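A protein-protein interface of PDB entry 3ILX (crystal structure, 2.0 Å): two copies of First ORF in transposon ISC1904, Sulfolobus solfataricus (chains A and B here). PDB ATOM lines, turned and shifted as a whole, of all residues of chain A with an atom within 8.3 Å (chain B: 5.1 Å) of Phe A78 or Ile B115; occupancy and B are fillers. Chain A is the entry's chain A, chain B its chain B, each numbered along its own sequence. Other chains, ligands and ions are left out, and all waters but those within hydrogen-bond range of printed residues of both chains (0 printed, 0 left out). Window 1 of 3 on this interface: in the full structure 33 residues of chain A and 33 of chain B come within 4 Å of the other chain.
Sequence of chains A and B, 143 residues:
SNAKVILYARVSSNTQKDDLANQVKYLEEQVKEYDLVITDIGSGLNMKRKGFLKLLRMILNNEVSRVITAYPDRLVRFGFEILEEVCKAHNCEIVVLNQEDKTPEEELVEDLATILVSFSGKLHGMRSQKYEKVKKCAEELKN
Phe B78 touches its own counterpart, Phe A78.
Ile B82 touches its own counterpart, Ile A82.
Leu A112 touches Leu B116, and with the chains exchanged Leu A116 touches Leu B112.
Ile A115 touches Phe B119, and with the chains exchanged Phe A119 touches Ile B115.
Positions printed for both chains: 45, 78, 82, 111, 112, 115, 116 and 119.
The side-chain carboxylate (OD2) of Asp A111 is in salt-bridge range of the guanidinium group (NE) of Arg A77 (2.9 Å).
N of Arg A77 is in hydrogen-bond range of O of Gly A44.
The guanidinium group of Arg A77 is in salt-bridge range of the side-chain carboxylate of Asp A73.
O of Leu B116 sits at hydrogen-bond distance from OG of Ser B120.
Among the printed residues, pairs that only touch across the chains: Phe A78 with Phe B78 (3.5 Å), Phe A52 with Ile B82 (3.8 Å), Ile A115 with Phe B119 (3.8 Å), Phe A119 with Leu B112 (3.8 Å), Arg A77 with Phe B119 (3.8 Å), Phe A119 with Ile B115 (3.9 Å), Leu A112 with Leu B116 (3.9 Å), Met A47 with Ile B82 (3.9 Å), Leu A116 with Leu B112 (3.9 Å), Leu A112 with Phe B119 (3.9 Å), Ile A82 with Ile B82 (3.9 Å) and Phe A78 with Ile B115 (3.99 Å).
Of the printed residues of chain B, Met A47 touches Ile B82 (3.9 Å).
Printed residues of chain B within 4 Å of Phe A78: Phe B78 and Ile B115.
Of the printed residues of chain B, Leu A116 touches Leu B112.
Of the printed residues of chain A, Phe B78 touches Phe A78.
Of the printed residues of chain A, Ile B82 touches Met A47, Phe A52 and Ile A82.
Of the printed residues of chain A, Ile B115 touches Phe A78 (3.99 Å) and Phe A119 (3.9 Å).
The nearest printed residue of chain B that does not touch Phe A78 is Leu B45 (4.2 Å).
The nearest printed residue of chain B that does not touch Leu A112 is Ile B115 (4.2 Å).
Hydrophobic or aromatic side chains of chain B within 4 Å of the printed part of chain A: Phe B78, Ile B82, Leu B112, Ile B115, Leu B116 and Phe B119.
Hydrophobic or aromatic side chains of chain A within 4 Å of the printed part of chain B: Met A47, Phe A52, Phe A78, Ile A82, Leu A112, Ile A115, Leu A116 and Phe A119.
Among the printed residues, 12 pairs touch across the chains.
Among the printed residues, no Asp or Glu carboxylate lies within 4 Å of a Lys or Arg side-chain nitrogen of the other chain.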
ATOM      1  N   GLY A  44      -2.033  -5.376  24.197  1.00  0.00           N
ATOM      2  CA  GLY A  44      -0.915  -4.456  23.983  1.00  0.00           C
ATOM      3  C   GLY A  44       0.000  -4.820  22.819  1.00  0.00           C
ATOM      4  O   GLY A  44       0.738  -3.950  22.315  1.00  0.00           O
ATOM      5  N   LEU A  45      -0.035  -6.082  22.393  1.00  0.00           N
ATOM      6  CA  LEU A  45       0.705  -6.531  21.215  1.00  0.00           C
ATOM      7  C   LEU A  45       0.044  -6.098  19.904  1.00  0.00           C
ATOM      8  O   LEU A  45       0.669  -6.187  18.843  1.00  0.00           O
ATOM      9  CB  LEU A  45       0.789  -8.070  21.181  1.00  0.00           C
ATOM     10  CG  LEU A  45       1.763  -8.714  22.158  1.00  0.00           C
ATOM     11  CD1 LEU A  45       1.516 -10.194  22.231  1.00  0.00           C
ATOM     12  CD2 LEU A  45       3.207  -8.439  21.692  1.00  0.00           C
ATOM     13  N   ASN A  46      -1.234  -5.708  19.958  1.00  0.00           N
ATOM     14  CA  ASN A  46      -1.996  -5.482  18.706  1.00  0.00           C
ATOM     15  C   ASN A  46      -1.697  -4.074  18.165  1.00  0.00           C
ATOM     16  O   ASN A  46      -2.105  -3.055  18.746  1.00  0.00           O
ATOM     17  CB  ASN A  46      -3.488  -5.735  18.928  1.00  0.00           C
ATOM     18  CG  ASN A  46      -4.359  -5.423  17.688  1.00  0.00           C
ATOM     19  OD1 ASN A  46      -3.872  -5.012  16.634  1.00  0.00           O
ATOM     20  ND2 ASN A  46      -5.661  -5.615  17.839  1.00  0.00           N
ATOM     21  N   MET A  47      -0.922  -4.035  17.092  1.00  0.00           N
ATOM     22  CA  MET A  47      -0.467  -2.773  16.491  1.00  0.00           C
ATOM     23  C   MET A  47      -1.553  -2.108  15.601  1.00  0.00           C
ATOM     24  O   MET A  47      -1.342  -1.007  15.067  1.00  0.00           O
ATOM     25  CB  MET A  47       0.812  -3.005  15.682  1.00  0.00           C
ATOM     26  CG  MET A  47       1.961  -3.591  16.470  1.00  0.00           C
ATOM     27  SD  MET A  47       2.701  -2.192  17.545  1.00  0.00           S
ATOM     28  CE  MET A  47       1.545  -2.345  19.120  1.00  0.00           C
ATOM     29  N   ARG A  49      -4.714  -1.564  16.948  1.00  0.00           N
ATOM     30  CA  ARG A  49      -5.673  -0.907  17.856  1.00  0.00           C
ATOM     31  C   ARG A  49      -5.999   0.520  17.362  1.00  0.00           C
ATOM     32  O   ARG A  49      -5.098   1.362  17.224  1.00  0.00           O
ATOM     33  CB  ARG A  49      -5.095  -0.808  19.267  1.00  0.00           C
ATOM     34  CG  ARG A  49      -5.236  -2.040  20.166  1.00  0.00           C
ATOM     35  CD  ARG A  49      -4.499  -1.793  21.506  1.00  0.00           C
ATOM     36  NE  ARG A  49      -3.069  -1.797  21.284  1.00  0.00           N
ATOM     37  CZ  ARG A  49      -2.186  -1.102  21.993  1.00  0.00           C
ATOM     38  NH1 ARG A  49      -0.901  -1.206  21.702  1.00  0.00           N
ATOM     39  NH2 ARG A  49      -2.563  -0.298  22.978  1.00  0.00           N
ATOM     40  N   PHE A  52      -5.066   3.307  19.969  1.00  0.00           N
ATOM     41  CA  PHE A  52      -3.615   3.512  20.125  1.00  0.00           C
ATOM     42  C   PHE A  52      -3.028   4.223  18.914  1.00  0.00           C
ATOM     43  O   PHE A  52      -2.167   5.093  19.067  1.00  0.00           O
ATOM     44  CB  PHE A  52      -2.920   2.167  20.326  1.00  0.00           C
ATOM     45  CG  PHE A  52      -1.407   2.209  20.219  1.00  0.00           C
ATOM     46  CD1 PHE A  52      -0.624   2.575  21.314  1.00  0.00           C
ATOM     47  CD2 PHE A  52      -0.770   1.774  19.051  1.00  0.00           C
ATOM     48  CE1 PHE A  52       0.772   2.593  21.201  1.00  0.00           C
ATOM     49  CE2 PHE A  52       0.602   1.748  18.960  1.00  0.00           C
ATOM     50  CZ  PHE A  52       1.379   2.159  20.070  1.00  0.00           C
ATOM     51  N   PRO A  72       2.600   1.127  32.485  1.00  0.00           N
ATOM     52  CA  PRO A  72       3.186   1.169  31.135  1.00  0.00           C
ATOM     53  C   PRO A  72       2.583   0.156  30.127  1.00  0.00           C
ATOM     54  O   PRO A  72       2.344   0.527  28.949  1.00  0.00           O
ATOM     55  CB  PRO A  72       4.692   0.907  31.386  1.00  0.00           C
ATOM     56  CG  PRO A  72       4.913   1.456  32.857  1.00  0.00           C
ATOM     57  CD  PRO A  72       3.629   1.022  33.549  1.00  0.00           C
ATOM     58  N   ASP A  73       2.297  -1.081  30.576  1.00  0.00           N
ATOM     59  CA  ASP A  73       1.779  -2.106  29.622  1.00  0.00           C
ATOM     60  C   ASP A  73       0.341  -1.855  29.148  1.00  0.00           C
ATOM     61  O   ASP A  73      -0.128  -2.496  28.198  1.00  0.00           O
ATOM     62  CB  ASP A  73       2.006  -3.552  30.098  1.00  0.00           C
ATOM     63  CG  ASP A  73       0.872  -4.084  30.954  1.00  0.00           C
ATOM     64  OD1 ASP A  73       0.036  -3.278  31.428  1.00  0.00           O
ATOM     65  OD2 ASP A  73       0.824  -5.321  31.172  1.00  0.00           O
ATOM     66  N   LEU A  75      -0.218   0.804  27.467  1.00  0.00           N
ATOM     67  CA  LEU A  75       0.080   1.342  26.120  1.00  0.00           C
ATOM     68  C   LEU A  75       0.553   0.279  25.158  1.00  0.00           C
ATOM     69  O   LEU A  75       0.024   0.163  24.047  1.00  0.00           O
ATOM     70  CB  LEU A  75       1.084   2.525  26.158  1.00  0.00           C
ATOM     71  CG  LEU A  75       0.356   3.839  26.483  1.00  0.00           C
ATOM     72  CD1 LEU A  75       1.335   4.942  26.992  1.00  0.00           C
ATOM     73  CD2 LEU A  75      -0.508   4.316  25.285  1.00  0.00           C
ATOM     74  N   VAL A  76       1.581  -0.465  25.554  1.00  0.00           N
ATOM     75  CA  VAL A  76       2.170  -1.505  24.705  1.00  0.00           C
ATOM     76  C   VAL A  76       2.807  -2.569  25.563  1.00  0.00           C
ATOM     77  O   VAL A  76       3.190  -2.306  26.725  1.00  0.00           O
ATOM     78  CB  VAL A  76       3.307  -0.967  23.761  1.00  0.00           C
ATOM     79  CG1 VAL A  76       2.731  -0.211  22.566  1.00  0.00           C
ATOM     80  CG2 VAL A  76       4.307  -0.094  24.536  1.00  0.00           C
ATOM     81  N   ARG A  77       2.956  -3.756  24.996  1.00  0.00           N
ATOM     82  CA  ARG A  77       3.706  -4.834  25.652  1.00  0.00           C
ATOM     83  C   ARG A  77       5.214  -4.683  25.385  1.00  0.00           C
ATOM     84  O   ARG A  77       6.019  -5.023  26.222  1.00  0.00           O
ATOM     85  CB  ARG A  77       3.179  -6.190  25.153  1.00  0.00           C
ATOM     86  CG  ARG A  77       3.966  -7.462  25.558  1.00  0.00           C
ATOM     87  CD  ARG A  77       3.941  -7.705  27.048  1.00  0.00           C
ATOM     88  NE  ARG A  77       2.566  -7.829  27.538  1.00  0.00           N
ATOM     89  CZ  ARG A  77       2.131  -7.413  28.734  1.00  0.00           C
ATOM     90  NH1 ARG A  77       2.955  -6.842  29.631  1.00  0.00           N
ATOM     91  NH2 ARG A  77       0.843  -7.567  29.040  1.00  0.00           N
ATOM     92  N   PHE A  78       5.587  -4.206  24.205  1.00  0.00           N
ATOM     93  CA  PHE A  78       7.011  -3.991  23.867  1.00  0.00           C
ATOM     94  C   PHE A  78       7.121  -2.592  23.312  1.00  0.00           C
ATOM     95  O   PHE A  78       6.178  -2.145  22.671  1.00  0.00           O
ATOM     96  CB  PHE A  78       7.466  -4.954  22.749  1.00  0.00           C
ATOM     97  CG  PHE A  78       7.565  -6.393  23.191  1.00  0.00           C
ATOM     98  CD1 PHE A  78       8.624  -6.812  24.015  1.00  0.00           C
ATOM     99  CD2 PHE A  78       6.600  -7.314  22.799  1.00  0.00           C
ATOM    100  CE1 PHE A  78       8.722  -8.160  24.449  1.00  0.00           C
ATOM    101  CE2 PHE A  78       6.668  -8.678  23.219  1.00  0.00           C
ATOM    102  CZ  PHE A  78       7.732  -9.099  24.051  1.00  0.00           C
ATOM    103  N   GLY A  79       8.272  -1.938  23.496  1.00  0.00           N
ATOM    104  CA  GLY A  79       8.564  -0.661  22.820  1.00  0.00           C
ATOM    105  C   GLY A  79       8.094   0.556  23.586  1.00  0.00           C
ATOM    106  O   GLY A  79       8.109   1.692  23.061  1.00  0.00           O
ATOM    107  N   PHE A  80       7.697   0.365  24.836  1.00  0.00           N
ATOM    108  CA  PHE A  80       7.378   1.545  25.647  1.00  0.00           C
ATOM    109  C   PHE A  80       8.475   2.634  25.518  1.00  0.00           C
ATOM    110  O   PHE A  80       8.176   3.818  25.419  1.00  0.00           O
ATOM    111  CB  PHE A  80       7.083   1.170  27.112  1.00  0.00           C
ATOM    112  CG  PHE A  80       6.527   2.317  27.932  1.00  0.00           C
ATOM    113  CD1 PHE A  80       5.177   2.596  27.936  1.00  0.00           C
ATOM    114  CD2 PHE A  80       7.373   3.106  28.699  1.00  0.00           C
ATOM    115  CE1 PHE A  80       4.651   3.643  28.709  1.00  0.00           C
ATOM    116  CE2 PHE A  80       6.863   4.188  29.490  1.00  0.00           C
ATOM    117  CZ  PHE A  80       5.512   4.458  29.487  1.00  0.00           C
ATOM    118  N   GLU A  81       9.727   2.218  25.442  1.00  0.00           N
ATOM    119  CA  GLU A  81      10.858   3.145  25.340  1.00  0.00           C
ATOM    120  C   GLU A  81      10.825   3.893  24.025  1.00  0.00           C
ATOM    121  O   GLU A  81      11.170   5.053  23.989  1.00  0.00           O
ATOM    122  CB  GLU A  81      12.194   2.430  25.468  1.00  0.00           C
ATOM    123  CG  GLU A  81      12.414   1.702  26.799  1.00  0.00           C
ATOM    124  CD  GLU A  81      11.866   0.273  26.809  1.00  0.00           C
ATOM    125  OE1 GLU A  81      10.994  -0.122  25.973  1.00  0.00           O
ATOM    126  OE2 GLU A  81      12.324  -0.454  27.696  1.00  0.00           O
ATOM    127  N   ILE A  82      10.417   3.234  22.934  1.00  0.00           N
ATOM    128  CA  ILE A  82      10.278   3.946  21.663  1.00  0.00           C
ATOM    129  C   ILE A  82       9.203   5.029  21.836  1.00  0.00           C
ATOM    130  O   ILE A  82       9.411   6.177  21.467  1.00  0.00           O
ATOM    131  CB  ILE A  82       9.935   2.986  20.479  1.00  0.00           C
ATOM    132  CG1 ILE A  82      11.129   2.079  20.190  1.00  0.00           C
ATOM    133  CG2 ILE A  82       9.528   3.789  19.188  1.00  0.00           C
ATOM    134  CD1 ILE A  82      10.718   0.825  19.420  1.00  0.00           C
ATOM    135  N   LEU A  83       8.074   4.686  22.447  1.00  0.00           N
ATOM    136  CA  LEU A  83       7.034   5.707  22.630  1.00  0.00           C
ATOM    137  C   LEU A  83       7.521   6.917  23.404  1.00  0.00           C
ATOM    138  O   LEU A  83       7.134   8.045  23.100  1.00  0.00           O
ATOM    139  CB  LEU A  83       5.781   5.143  23.309  1.00  0.00           C
ATOM    140  CG  LEU A  83       5.100   4.039  22.516  1.00  0.00           C
ATOM    141  CD1 LEU A  83       3.939   3.518  23.360  1.00  0.00           C
ATOM    142  CD2 LEU A  83       4.577   4.551  21.146  1.00  0.00           C
ATOM    143  N   ASP A 111      -0.817 -13.144  25.955  1.00  0.00           N
ATOM    144  CA  ASP A 111       0.247 -12.458  25.200  1.00  0.00           C
ATOM    145  C   ASP A 111       1.429 -13.402  24.919  1.00  0.00           C
ATOM    146  O   ASP A 111       1.950 -13.467  23.787  1.00  0.00           O
ATOM    147  CB  ASP A 111       0.724 -11.214  25.958  1.00  0.00           C
ATOM    148  CG  ASP A 111      -0.189 -10.001  25.750  1.00  0.00           C
ATOM    149  OD1 ASP A 111      -1.180 -10.063  24.951  1.00  0.00           O
ATOM    150  OD2 ASP A 111       0.118  -8.955  26.382  1.00  0.00           O
ATOM    151  N   LEU A 112       1.830 -14.166  25.930  1.00  0.00           N
ATOM    152  CA  LEU A 112       2.870 -15.172  25.710  1.00  0.00           C
ATOM    153  C   LEU A 112       2.464 -16.212  24.640  1.00  0.00           C
ATOM    154  O   LEU A 112       3.266 -16.542  23.770  1.00  0.00           O
ATOM    155  CB  LEU A 112       3.298 -15.836  27.009  1.00  0.00           C
ATOM    156  CG  LEU A 112       4.598 -16.652  26.933  1.00  0.00           C
ATOM    157  CD1 LEU A 112       5.752 -15.912  26.229  1.00  0.00           C
ATOM    158  CD2 LEU A 112       4.992 -17.002  28.358  1.00  0.00           C
ATOM    159  N   ILE A 115       2.899 -14.654  21.304  1.00  0.00           N
ATOM    160  CA  ILE A 115       4.327 -14.539  21.030  1.00  0.00           C
ATOM    161  C   ILE A 115       4.905 -15.933  20.638  1.00  0.00           C
ATOM    162  O   ILE A 115       5.648 -16.047  19.655  1.00  0.00           O
ATOM    163  CB  ILE A 115       5.088 -13.956  22.271  1.00  0.00           C
ATOM    164  CG1 ILE A 115       4.748 -12.467  22.493  1.00  0.00           C
ATOM    165  CG2 ILE A 115       6.612 -14.115  22.133  1.00  0.00           C
ATOM    166  CD1 ILE A 115       5.058 -11.999  23.959  1.00  0.00           C
ATOM    167  N   LEU A 116       4.537 -16.971  21.401  1.00  0.00           N
ATOM    168  CA  LEU A 116       5.002 -18.353  21.162  1.00  0.00           C
ATOM    169  C   LEU A 116       4.577 -18.860  19.796  1.00  0.00           C
ATOM    170  O   LEU A 116       5.390 -19.442  19.079  1.00  0.00           O
ATOM    171  CB  LEU A 116       4.508 -19.317  22.251  1.00  0.00           C
ATOM    172  CG  LEU A 116       5.214 -19.089  23.598  1.00  0.00           C
ATOM    173  CD1 LEU A 116       4.501 -19.859  24.690  1.00  0.00           C
ATOM    174  CD2 LEU A 116       6.678 -19.459  23.542  1.00  0.00           C
ATOM    175  N   PHE A 119       6.846 -17.133  17.147  1.00  0.00           N
ATOM    176  CA  PHE A 119       8.161 -17.771  17.071  1.00  0.00           C
ATOM    177  C   PHE A 119       8.108 -19.189  16.454  1.00  0.00           C
ATOM    178  O   PHE A 119       8.955 -19.540  15.615  1.00  0.00           O
ATOM    179  CB  PHE A 119       8.803 -17.799  18.463  1.00  0.00           C
ATOM    180  CG  PHE A 119       9.550 -16.540  18.804  1.00  0.00           C
ATOM    181  CD1 PHE A 119      10.926 -16.455  18.585  1.00  0.00           C
ATOM    182  CD2 PHE A 119       8.870 -15.418  19.264  1.00  0.00           C
ATOM    183  CE1 PHE A 119      11.635 -15.281  18.884  1.00  0.00           C
ATOM    184  CE2 PHE A 119       9.567 -14.242  19.594  1.00  0.00           C
ATOM    185  CZ  PHE A 119      10.958 -14.168  19.385  1.00  0.00           C
ATOM    186  N   LEU B  45      15.467  -6.636  20.473  1.00  0.00           N
ATOM    187  CA  LEU B  45      14.620  -6.349  21.643  1.00  0.00           C
ATOM    188  C   LEU B  45      15.268  -5.271  22.506  1.00  0.00           C
ATOM    189  O   LEU B  45      14.624  -4.700  23.387  1.00  0.00           O
ATOM    190  CB  LEU B  45      14.423  -7.608  22.546  1.00  0.00           C
ATOM    191  CG  LEU B  45      13.645  -8.803  21.992  1.00  0.00           C
ATOM    192  CD1 LEU B  45      13.936 -10.071  22.841  1.00  0.00           C
ATOM    193  CD2 LEU B  45      12.121  -8.506  21.931  1.00  0.00           C
ATOM    194  N   PHE B  78       9.978  -6.407  17.705  1.00  0.00           N
ATOM    195  CA  PHE B  78       8.583  -6.011  17.823  1.00  0.00           C
ATOM    196  C   PHE B  78       8.453  -4.529  17.566  1.00  0.00           C
ATOM    197  O   PHE B  78       9.394  -3.778  17.830  1.00  0.00           O
ATOM    198  CB  PHE B  78       8.040  -6.301  19.254  1.00  0.00           C
ATOM    199  CG  PHE B  78       7.853  -7.766  19.538  1.00  0.00           C
ATOM    200  CD1 PHE B  78       6.746  -8.431  19.049  1.00  0.00           C
ATOM    201  CD2 PHE B  78       8.803  -8.469  20.297  1.00  0.00           C
ATOM    202  CE1 PHE B  78       6.557  -9.783  19.306  1.00  0.00           C
ATOM    203  CE2 PHE B  78       8.646  -9.828  20.553  1.00  0.00           C
ATOM    204  CZ  PHE B  78       7.522 -10.492  20.057  1.00  0.00           C
ATOM    205  N   ILE B  82       5.135   0.795  14.725  1.00  0.00           N
ATOM    206  CA  ILE B  82       5.307   2.083  15.353  1.00  0.00           C
ATOM    207  C   ILE B  82       6.395   2.902  14.640  1.00  0.00           C
ATOM    208  O   ILE B  82       6.208   4.108  14.390  1.00  0.00           O
ATOM    209  CB  ILE B  82       5.617   1.939  16.850  1.00  0.00           C
ATOM    210  CG1 ILE B  82       4.385   1.410  17.588  1.00  0.00           C
ATOM    211  CG2 ILE B  82       6.022   3.295  17.452  1.00  0.00           C
ATOM    212  CD1 ILE B  82       4.733   0.836  18.960  1.00  0.00           C
ATOM    213  N   ASP B 111      16.311 -14.556  21.602  1.00  0.00           N
ATOM    214  CA  ASP B 111      15.229 -13.563  21.812  1.00  0.00           C
ATOM    215  C   ASP B 111      14.019 -14.142  22.557  1.00  0.00           C
ATOM    216  O   ASP B 111      13.500 -13.518  23.518  1.00  0.00           O
ATOM    217  CB  ASP B 111      14.783 -12.965  20.471  1.00  0.00           C
ATOM    218  CG  ASP B 111      15.718 -11.833  19.985  1.00  0.00           C
ATOM    219  OD1 ASP B 111      16.793 -11.608  20.608  1.00  0.00           O
ATOM    220  OD2 ASP B 111      15.378 -11.182  18.970  1.00  0.00           O
ATOM    221  N   LEU B 112      13.597 -15.340  22.142  1.00  0.00           N
ATOM    222  CA  LEU B 112      12.514 -16.064  22.840  1.00  0.00           C
ATOM    223  C   LEU B 112      12.837 -16.266  24.339  1.00  0.00           C
ATOM    224  O   LEU B 112      12.001 -15.968  25.208  1.00  0.00           O
ATOM    225  CB  LEU B 112      12.182 -17.397  22.147  1.00  0.00           C
ATOM    226  CG  LEU B 112      10.917 -18.089  22.669  1.00  0.00           C
ATOM    227  CD1 LEU B 112       9.748 -17.108  22.837  1.00  0.00           C
ATOM    228  CD2 LEU B 112      10.506 -19.252  21.775  1.00  0.00           C
ATOM    229  N   ALA B 113      14.052 -16.744  24.606  1.00  0.00           N
ATOM    230  CA  ALA B 113      14.555 -16.962  25.957  1.00  0.00           C
ATOM    231  C   ALA B 113      14.522 -15.692  26.803  1.00  0.00           C
ATOM    232  O   ALA B 113      14.128 -15.752  27.984  1.00  0.00           O
ATOM    233  CB  ALA B 113      15.988 -17.535  25.918  1.00  0.00           C
ATOM    234  N   THR B 114      14.971 -14.571  26.227  1.00  0.00           N
ATOM    235  CA  THR B 114      14.867 -13.251  26.875  1.00  0.00           C
ATOM    236  C   THR B 114      13.423 -12.951  27.235  1.00  0.00           C
ATOM    237  O   THR B 114      13.134 -12.515  28.352  1.00  0.00           O
ATOM    238  CB  THR B 114      15.411 -12.077  25.984  1.00  0.00           C
ATOM    239  OG1 THR B 114      16.807 -12.269  25.724  1.00  0.00           O
ATOM    240  CG2 THR B 114      15.204 -10.708  26.670  1.00  0.00           C
ATOM    241  N   ILE B 115      12.518 -13.182  26.289  1.00  0.00           N
ATOM    242  CA  ILE B 115      11.111 -12.878  26.520  1.00  0.00           C
ATOM    243  C   ILE B 115      10.520 -13.765  27.645  1.00  0.00           C
ATOM    244  O   ILE B 115       9.827 -13.273  28.545  1.00  0.00           O
ATOM    245  CB  ILE B 115      10.284 -12.999  25.204  1.00  0.00           C
ATOM    246  CG1 ILE B 115      10.620 -11.852  24.234  1.00  0.00           C
ATOM    247  CG2 ILE B 115       8.778 -13.044  25.482  1.00  0.00           C
ATOM    248  CD1 ILE B 115      10.198 -12.190  22.796  1.00  0.00           C
ATOM    249  N   LEU B 116      10.836 -15.070  27.587  1.00  0.00           N
ATOM    250  CA  LEU B 116      10.332 -16.039  28.566  1.00  0.00           C
ATOM    251  C   LEU B 116      10.806 -15.725  29.958  1.00  0.00           C
ATOM    252  O   LEU B 116      10.006 -15.804  30.891  1.00  0.00           O
ATOM    253  CB  LEU B 116      10.738 -17.465  28.192  1.00  0.00           C
ATOM    254  CG  LEU B 116       9.967 -17.977  26.973  1.00  0.00           C
ATOM    255  CD1 LEU B 116      10.715 -19.184  26.472  1.00  0.00           C
ATOM    256  CD2 LEU B 116       8.574 -18.362  27.350  1.00  0.00           C
ATOM    257  N   VAL B 117      12.095 -15.375  30.095  1.00  0.00           N
ATOM    258  CA  VAL B 117      12.619 -14.922  31.386  1.00  0.00           C
ATOM    259  C   VAL B 117      11.845 -13.696  31.862  1.00  0.00           C
ATOM    260  O   VAL B 117      11.510 -13.594  33.043  1.00  0.00           O
ATOM    261  CB  VAL B 117      14.133 -14.549  31.339  1.00  0.00           C
ATOM    262  CG1 VAL B 117      14.566 -13.856  32.650  1.00  0.00           C
ATOM    263  CG2 VAL B 117      14.991 -15.787  31.080  1.00  0.00           C
ATOM    264  N   SER B 118      11.622 -12.743  30.954  1.00  0.00           N
ATOM    265  CA  SER B 118      10.852 -11.548  31.288  1.00  0.00           C
ATOM    266  C   SER B 118       9.459 -11.938  31.839  1.00  0.00           C
ATOM    267  O   SER B 118       9.090 -11.547  32.930  1.00  0.00           O
ATOM    268  CB  SER B 118      10.740 -10.604  30.064  1.00  0.00           C
ATOM    269  OG  SER B 118       9.992  -9.455  30.427  1.00  0.00           O
ATOM    270  N   PHE B 119       8.724 -12.756  31.092  1.00  0.00           N
ATOM    271  CA  PHE B 119       7.383 -13.212  31.517  1.00  0.00           C
ATOM    272  C   PHE B 119       7.387 -13.993  32.843  1.00  0.00           C
ATOM    273  O   PHE B 119       6.523 -13.776  33.696  1.00  0.00           O
ATOM    274  CB  PHE B 119       6.716 -14.013  30.403  1.00  0.00           C
ATOM    275  CG  PHE B 119       5.951 -13.153  29.450  1.00  0.00           C
ATOM    276  CD1 PHE B 119       4.558 -13.038  29.561  1.00  0.00           C
ATOM    277  CD2 PHE B 119       6.629 -12.381  28.488  1.00  0.00           C
ATOM    278  CE1 PHE B 119       3.843 -12.200  28.679  1.00  0.00           C
ATOM    279  CE2 PHE B 119       5.917 -11.544  27.606  1.00  0.00           C
ATOM    280  CZ  PHE B 119       4.522 -11.448  27.706  1.00  0.00           C
ATOM    281  N   SER B 120       8.371 -14.880  33.033  1.00  0.00           N
ATOM    282  CA  SER B 120       8.410 -15.619  34.307  1.00  0.00           C
ATOM    283  C   SER B 120       8.551 -14.659  35.472  1.00  0.00           C
ATOM    284  O   SER B 120       7.962 -14.884  36.524  1.00  0.00           O
ATOM    285  CB  SER B 120       9.486 -16.712  34.330  1.00  0.00           C
ATOM    286  OG  SER B 120      10.774 -16.179  34.124  1.00  0.00           O
